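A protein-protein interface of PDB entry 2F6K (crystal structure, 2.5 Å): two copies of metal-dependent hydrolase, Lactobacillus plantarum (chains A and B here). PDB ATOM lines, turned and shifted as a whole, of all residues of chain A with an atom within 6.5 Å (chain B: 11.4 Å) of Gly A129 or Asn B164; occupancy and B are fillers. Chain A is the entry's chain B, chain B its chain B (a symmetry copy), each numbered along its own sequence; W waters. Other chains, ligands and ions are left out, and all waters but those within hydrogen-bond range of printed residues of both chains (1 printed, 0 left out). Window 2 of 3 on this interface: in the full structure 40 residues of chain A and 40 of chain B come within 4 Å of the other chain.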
ATOM      1  N   ASN A  62     -12.359 -17.443  41.640  1.00  0.00           N
ATOM      2  CA  ASN A  62     -13.318 -18.411  41.129  1.00  0.00           C
ATOM      3  C   ASN A  62     -12.493 -19.582  40.611  1.00  0.00           C
ATOM      4  O   ASN A  62     -11.997 -19.541  39.491  1.00  0.00           O
ATOM      5  CB  ASN A  62     -14.127 -17.798  39.987  1.00  0.00           C
ATOM      6  CG  ASN A  62     -14.987 -18.818  39.260  1.00  0.00           C
ATOM      7  OD1 ASN A  62     -15.608 -18.505  38.246  1.00  0.00           O
ATOM      8  ND2 ASN A  62     -15.027 -20.038  39.775  1.00  0.00           N
ATOM      9  N   ASN A 126     -13.411 -10.668  33.506  1.00  0.00           N
ATOM     10  CA  ASN A 126     -14.017 -11.975  33.258  1.00  0.00           C
ATOM     11  C   ASN A 126     -13.597 -12.917  34.371  1.00  0.00           C
ATOM     12  O   ASN A 126     -12.456 -12.887  34.830  1.00  0.00           O
ATOM     13  CB  ASN A 126     -13.584 -12.551  31.897  1.00  0.00           C
ATOM     14  CG  ASN A 126     -12.328 -13.432  31.986  1.00  0.00           C
ATOM     15  OD1 ASN A 126     -12.355 -14.537  32.542  1.00  0.00           O
ATOM     16  ND2 ASN A 126     -11.224 -12.942  31.429  1.00  0.00           N
ATOM     17  N   SER A 127     -14.529 -13.737  34.829  1.00  0.00           N
ATOM     18  CA  SER A 127     -14.222 -14.702  35.869  1.00  0.00           C
ATOM     19  C   SER A 127     -14.406 -16.050  35.205  1.00  0.00           C
ATOM     20  O   SER A 127     -15.539 -16.467  34.962  1.00  0.00           O
ATOM     21  CB  SER A 127     -15.191 -14.566  37.038  1.00  0.00           C
ATOM     22  OG  SER A 127     -14.862 -15.487  38.059  1.00  0.00           O
ATOM     23  N   ARG A 128     -13.294 -16.712  34.890  1.00  0.00           N
ATOM     24  CA  ARG A 128     -13.324 -18.011  34.229  1.00  0.00           C
ATOM     25  C   ARG A 128     -14.306 -18.016  33.065  1.00  0.00           C
ATOM     26  O   ARG A 128     -15.083 -18.952  32.911  1.00  0.00           O
ATOM     27  CB  ARG A 128     -13.703 -19.133  35.212  1.00  0.00           C
ATOM     28  CG  ARG A 128     -12.654 -19.444  36.284  1.00  0.00           C
ATOM     29  CD  ARG A 128     -12.973 -20.762  36.997  1.00  0.00           C
ATOM     30  NE  ARG A 128     -12.689 -21.926  36.159  1.00  0.00           N
ATOM     31  CZ  ARG A 128     -11.496 -22.509  36.061  1.00  0.00           C
ATOM     32  NH1 ARG A 128     -10.467 -22.040  36.758  1.00  0.00           N
ATOM     33  NH2 ARG A 128     -11.324 -23.554  35.257  1.00  0.00           N
ATOM     34  N   GLY A 129     -14.288 -16.961  32.258  1.00  0.00           N
ATOM     35  CA  GLY A 129     -15.175 -16.923  31.112  1.00  0.00           C
ATOM     36  C   GLY A 129     -16.419 -16.063  31.199  1.00  0.00           C
ATOM     37  O   GLY A 129     -17.014 -15.754  30.167  1.00  0.00           O
ATOM     38  N   LEU A 130     -16.841 -15.689  32.407  1.00  0.00           N
ATOM     39  CA  LEU A 130     -18.024 -14.844  32.539  1.00  0.00           C
ATOM     40  C   LEU A 130     -17.587 -13.382  32.547  1.00  0.00           C
ATOM     41  O   LEU A 130     -17.128 -12.863  33.574  1.00  0.00           O
ATOM     42  CB  LEU A 130     -18.783 -15.176  33.819  1.00  0.00           C
ATOM     43  CG  LEU A 130     -20.165 -14.525  33.944  1.00  0.00           C
ATOM     44  CD1 LEU A 130     -20.909 -15.115  35.123  1.00  0.00           C
ATOM     45  CD2 LEU A 130     -20.031 -13.023  34.132  1.00  0.00           C
ATOM     46  N   TYR A 131     -17.736 -12.725  31.399  1.00  0.00           N
ATOM     47  CA  TYR A 131     -17.334 -11.330  31.259  1.00  0.00           C
ATOM     48  C   TYR A 131     -18.323 -10.331  31.838  1.00  0.00           C
ATOM     49  O   TYR A 131     -19.537 -10.452  31.655  1.00  0.00           O
ATOM     50  CB  TYR A 131     -17.062 -10.992  29.786  1.00  0.00           C
ATOM     51  CG  TYR A 131     -15.737 -11.524  29.288  1.00  0.00           C
ATOM     52  CD1 TYR A 131     -15.577 -12.877  28.982  1.00  0.00           C
ATOM     53  CD2 TYR A 131     -14.620 -10.692  29.199  1.00  0.00           C
ATOM     54  CE1 TYR A 131     -14.334 -13.388  28.609  1.00  0.00           C
ATOM     55  CE2 TYR A 131     -13.372 -11.194  28.830  1.00  0.00           C
ATOM     56  CZ  TYR A 131     -13.238 -12.542  28.541  1.00  0.00           C
ATOM     57  OH  TYR A 131     -12.006 -13.050  28.218  1.00  0.00           O
ATOM     58  N   SER A 134     -22.270  -9.209  31.313  1.00  0.00           N
ATOM     59  CA  SER A 134     -23.114 -10.365  31.041  1.00  0.00           C
ATOM     60  C   SER A 134     -24.444 -10.255  31.786  1.00  0.00           C
ATOM     61  O   SER A 134     -24.480  -9.917  32.973  1.00  0.00           O
ATOM     62  CB  SER A 134     -22.391 -11.658  31.419  1.00  0.00           C
ATOM     63  OG  SER A 134     -23.037 -12.788  30.857  1.00  0.00           O
ATOM     64  N   ALA A 159     -10.229 -15.390  28.859  1.00  0.00           N
ATOM     65  CA  ALA A 159     -10.730 -16.754  28.997  1.00  0.00           C
ATOM     66  C   ALA A 159      -9.931 -17.732  28.144  1.00  0.00           C
ATOM     67  O   ALA A 159      -9.495 -18.776  28.626  1.00  0.00           O
ATOM     68  CB  ALA A 159     -12.204 -16.808  28.619  1.00  0.00           C
ATOM     69  N   ASN A 186     -18.203  -5.271  25.494  1.00  0.00           N
ATOM     70  CA  ASN A 186     -19.271  -6.178  25.897  1.00  0.00           C
ATOM     71  C   ASN A 186     -20.342  -5.372  26.619  1.00  0.00           C
ATOM     72  O   ASN A 186     -21.535  -5.618  26.463  1.00  0.00           O
ATOM     73  CB  ASN A 186     -18.724  -7.255  26.833  1.00  0.00           C
ATOM     74  CG  ASN A 186     -19.657  -8.438  26.970  1.00  0.00           C
ATOM     75  OD1 ASN A 186     -20.027  -8.834  28.080  1.00  0.00           O
ATOM     76  ND2 ASN A 186     -20.034  -9.022  25.840  1.00  0.00           N
ATOM     77  N   TYR A 190     -24.443  -4.659  25.689  1.00  0.00           N
ATOM     78  CA  TYR A 190     -25.563  -4.896  26.589  1.00  0.00           C
ATOM     79  C   TYR A 190     -26.202  -3.636  27.182  1.00  0.00           C
ATOM     80  O   TYR A 190     -26.967  -3.712  28.140  1.00  0.00           O
ATOM     81  CB  TYR A 190     -25.124  -5.859  27.696  1.00  0.00           C
ATOM     82  CG  TYR A 190     -24.957  -7.271  27.191  1.00  0.00           C
ATOM     83  CD1 TYR A 190     -26.049  -7.971  26.681  1.00  0.00           C
ATOM     84  CD2 TYR A 190     -23.702  -7.888  27.152  1.00  0.00           C
ATOM     85  CE1 TYR A 190     -25.908  -9.250  26.135  1.00  0.00           C
ATOM     86  CE2 TYR A 190     -23.546  -9.175  26.601  1.00  0.00           C
ATOM     87  CZ  TYR A 190     -24.663  -9.844  26.093  1.00  0.00           C
ATOM     88  OH  TYR A 190     -24.545 -11.093  25.538  1.00  0.00           O
ATOM     89  N   ILE B 160      -8.334 -18.301  18.229  1.00  0.00           N
ATOM     90  CA  ILE B 160      -9.387 -18.600  19.185  1.00  0.00           C
ATOM     91  C   ILE B 160      -9.610 -17.446  20.164  1.00  0.00           C
ATOM     92  O   ILE B 160      -8.662 -16.766  20.578  1.00  0.00           O
ATOM     93  CB  ILE B 160      -9.068 -19.893  19.960  1.00  0.00           C
ATOM     94  CG1 ILE B 160     -10.359 -20.456  20.549  1.00  0.00           C
ATOM     95  CG2 ILE B 160      -8.042 -19.621  21.057  1.00  0.00           C
ATOM     96  CD1 ILE B 160     -10.164 -21.752  21.272  1.00  0.00           C
ATOM     97  N   LEU B 161     -10.873 -17.232  20.525  1.00  0.00           N
ATOM     98  CA  LEU B 161     -11.249 -16.157  21.437  1.00  0.00           C
ATOM     99  C   LEU B 161     -12.340 -16.579  22.405  1.00  0.00           C
ATOM    100  O   LEU B 161     -13.019 -17.584  22.195  1.00  0.00           O
ATOM    101  CB  LEU B 161     -11.752 -14.950  20.649  1.00  0.00           C
ATOM    102  CG  LEU B 161     -10.757 -14.230  19.743  1.00  0.00           C
ATOM    103  CD1 LEU B 161     -11.489 -13.172  18.945  1.00  0.00           C
ATOM    104  CD2 LEU B 161      -9.643 -13.611  20.571  1.00  0.00           C
ATOM    105  N   PRO B 162     -12.515 -15.816  23.493  1.00  0.00           N
ATOM    106  CA  PRO B 162     -13.564 -16.173  24.453  1.00  0.00           C
ATOM    107  C   PRO B 162     -14.878 -16.145  23.680  1.00  0.00           C
ATOM    108  O   PRO B 162     -15.076 -15.279  22.830  1.00  0.00           O
ATOM    109  CB  PRO B 162     -13.463 -15.064  25.496  1.00  0.00           C
ATOM    110  CG  PRO B 162     -11.989 -14.741  25.481  1.00  0.00           C
ATOM    111  CD  PRO B 162     -11.692 -14.703  23.996  1.00  0.00           C
ATOM    112  N   LYS B 163     -15.769 -17.086  23.957  1.00  0.00           N
ATOM    113  CA  LYS B 163     -17.029 -17.139  23.230  1.00  0.00           C
ATOM    114  C   LYS B 163     -18.165 -16.364  23.847  1.00  0.00           C
ATOM    115  O   LYS B 163     -19.116 -16.023  23.153  1.00  0.00           O
ATOM    116  CB  LYS B 163     -17.468 -18.592  23.033  1.00  0.00           C
ATOM    117  CG  LYS B 163     -16.581 -19.333  22.051  1.00  0.00           C
ATOM    118  CD  LYS B 163     -17.166 -20.668  21.627  1.00  0.00           C
ATOM    119  CE  LYS B 163     -16.250 -21.355  20.623  1.00  0.00           C
ATOM    120  NZ  LYS B 163     -16.818 -22.655  20.183  1.00  0.00           N
ATOM    121  N   ASN B 164     -18.086 -16.092  25.143  1.00  0.00           N
ATOM    122  CA  ASN B 164     -19.155 -15.359  25.804  1.00  0.00           C
ATOM    123  C   ASN B 164     -18.844 -13.889  26.041  1.00  0.00           C
ATOM    124  O   ASN B 164     -19.077 -13.356  27.126  1.00  0.00           O
ATOM    125  CB  ASN B 164     -19.512 -16.053  27.113  1.00  0.00           C
ATOM    126  CG  ASN B 164     -20.119 -17.406  26.876  1.00  0.00           C
ATOM    127  OD1 ASN B 164     -21.084 -17.522  26.128  1.00  0.00           O
ATOM    128  ND2 ASN B 164     -19.559 -18.437  27.496  1.00  0.00           N
ATOM    129  N   VAL B 165     -18.314 -13.236  25.013  1.00  0.00           N
ATOM    130  CA  VAL B 165     -17.991 -11.822  25.101  1.00  0.00           C
ATOM    131  C   VAL B 165     -18.042 -11.251  23.692  1.00  0.00           C
ATOM    132  O   VAL B 165     -17.699 -11.941  22.738  1.00  0.00           O
ATOM    133  CB  VAL B 165     -16.593 -11.602  25.731  1.00  0.00           C
ATOM    134  CG1 VAL B 165     -15.503 -12.058  24.770  1.00  0.00           C
ATOM    135  CG2 VAL B 165     -16.430 -10.141  26.126  1.00  0.00           C
ATOM    136  N   ASP B 166     -18.494 -10.004  23.568  1.00  0.00           N
ATOM    137  CA  ASP B 166     -18.614  -9.333  22.270  1.00  0.00           C
ATOM    138  C   ASP B 166     -19.337 -10.211  21.244  1.00  0.00           C
ATOM    139  O   ASP B 166     -19.059 -10.127  20.045  1.00  0.00           O
ATOM    140  CB  ASP B 166     -17.233  -8.968  21.708  1.00  0.00           C
ATOM    141  CG  ASP B 166     -16.344  -8.274  22.724  1.00  0.00           C
ATOM    142  OD1 ASP B 166     -16.813  -7.318  23.379  1.00  0.00           O
ATOM    143  OD2 ASP B 166     -15.165  -8.682  22.851  1.00  0.00           O
ATOM    144  N   ILE B 167     -20.259 -11.048  21.709  1.00  0.00           N
ATOM    145  CA  ILE B 167     -20.991 -11.945  20.819  1.00  0.00           C
ATOM    146  C   ILE B 167     -21.494 -11.278  19.534  1.00  0.00           C
ATOM    147  O   ILE B 167     -22.231 -10.287  19.573  1.00  0.00           O
ATOM    148  CB  ILE B 167     -22.174 -12.620  21.564  1.00  0.00           C
ATOM    149  CG1 ILE B 167     -21.636 -13.668  22.547  1.00  0.00           C
ATOM    150  CG2 ILE B 167     -23.137 -13.275  20.561  1.00  0.00           C
ATOM    151  CD1 ILE B 167     -22.714 -14.353  23.337  1.00  0.00           C
ATOM    152  N   ASP B 168     -21.060 -11.836  18.402  1.00  0.00           N
ATOM    153  CA  ASP B 168     -21.425 -11.370  17.064  1.00  0.00           C
ATOM    154  C   ASP B 168     -20.793 -10.049  16.612  1.00  0.00           C
ATOM    155  O   ASP B 168     -21.222  -9.455  15.624  1.00  0.00           O
ATOM    156  CB  ASP B 168     -22.956 -11.302  16.922  1.00  0.00           C
ATOM    157  CG  ASP B 168     -23.604 -12.684  16.887  1.00  0.00           C
ATOM    158  OD1 ASP B 168     -23.023 -13.597  16.262  1.00  0.00           O
ATOM    159  OD2 ASP B 168     -24.695 -12.858  17.470  1.00  0.00           O
ATOM    160  N   LEU B 169     -19.778  -9.586  17.333  1.00  0.00           N
ATOM    161  CA  LEU B 169     -19.088  -8.357  16.952  1.00  0.00           C
ATOM    162  C   LEU B 169     -18.241  -8.742  15.743  1.00  0.00           C
ATOM    163  O   LEU B 169     -17.427  -9.656  15.832  1.00  0.00           O
ATOM    164  CB  LEU B 169     -18.170  -7.881  18.082  1.00  0.00           C
ATOM    165  CG  LEU B 169     -17.411  -6.573  17.857  1.00  0.00           C
ATOM    166  CD1 LEU B 169     -18.381  -5.405  17.931  1.00  0.00           C
ATOM    167  CD2 LEU B 169     -16.337  -6.414  18.913  1.00  0.00           C
ATOM    168  N   LEU B 174     -12.453  -5.525  16.063  1.00  0.00           N
ATOM    169  CA  LEU B 174     -11.535  -5.670  17.189  1.00  0.00           C
ATOM    170  C   LEU B 174     -10.586  -6.860  17.028  1.00  0.00           C
ATOM    171  O   LEU B 174      -9.420  -6.785  17.412  1.00  0.00           O
ATOM    172  CB  LEU B 174     -12.333  -5.804  18.497  1.00  0.00           C
ATOM    173  CG  LEU B 174     -11.578  -6.180  19.780  1.00  0.00           C
ATOM    174  CD1 LEU B 174     -10.533  -5.126  20.115  1.00  0.00           C
ATOM    175  CD2 LEU B 174     -12.575  -6.315  20.923  1.00  0.00           C
HETATM  176  O   HOH W   1     -16.391 -16.391  27.398  1.00  0.00           O
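Among the printed residues, merely in contact across the chains: Tyr A131 with Pro B162 (3.2 Å), Tyr A131 with Val B165 (3.5 Å), Asn A186 with Val B165 (3.5 Å), Ala A159 with Pro B162 (3.8 Å), Gly A129 with Asn B164 (3.96 Å) and Tyr A131 with Asn B164 (3.99 Å).
The side-chain amide nitrogen of Asn A186 lies close to the backbone NH of Asp B166 (2.9 Å).
Water W1 lies within hydrogen-bond range of the backbone NH of Asn B164 (2.8 Å) and the backbone carbonyl oxygen of Gly A129 (2.9 Å).
The backbone NH (N) of Ala A159 lies within hydrogen-bond range of the side-chain hydroxyl (OH) of Tyr A131 (3.0 Å).
The side-chain amide nitrogen (ND2) of Asn A126 lies within hydrogen-bond range of the side-chain hydroxyl (OH) of Tyr A131 (3.3 Å).
N of Gly A129 lies within hydrogen-bond range of OD1 of Asn A126 (3.1 Å).
No position is printed for both chains.
Of the 7 pairs that touch across the chains among the printed residues, none has its exchanged pair printed and touching as well.
Of the 11 printed residues of chain A, 4 touch a printed residue of chain B.
Of the 11 printed residues of chain B, 4 touch a printed residue of chain A.
Printed residues of chain B that touch a printed residue of chain A: Pro B162, Asn B164, Val B165 and Asp B166.
Hydrophobic or aromatic side chains of chain B that line the printed part of chain A: Pro B162 and Val B165.
Among the printed residues, 7 pairs touch across the chains.
Gly A129 touches just one residue of chain B: Asn B164 (3.96 Å).
Printed residues of chain A within 4 Å of Asn B164: Gly A129 (3.96 Å) and Tyr A131 (3.99 Å).
No residue of chain B comes within 4 Å of Asn A126.
Ser A127 touches none of the printed residues of chain B.
No residue of chain B comes within 4 Å of Leu A130.
Ala A159 touches just one residue of chain B: Pro B162.
Of the printed residues of chain B, Asn A186 touches Val B165 (3.5 Å) and Asp B166 (2.9 Å).
Printed residues of chain A within 4 Å of Val B165: Tyr A131 and Asn A186.
Of the printed residues of chain B, Tyr A131 touches Pro B162 (3.2 Å), Asn B164 (3.99 Å) and Val B165 (3.5 Å).
Printed residues of chain A within 4 Å of Pro B162: Tyr A131 and Ala A159.
Tyr A190 touches none of the printed residues of chain B.
Asp B168 touches none of the printed residues of chain A.
The nearest printed residue of chain B that does not touch Gly A129 is Val B165 (5.9 Å).
The nearest printed residue of chain A that does not touch Val B165 is Gly A129 (5.9 Å).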
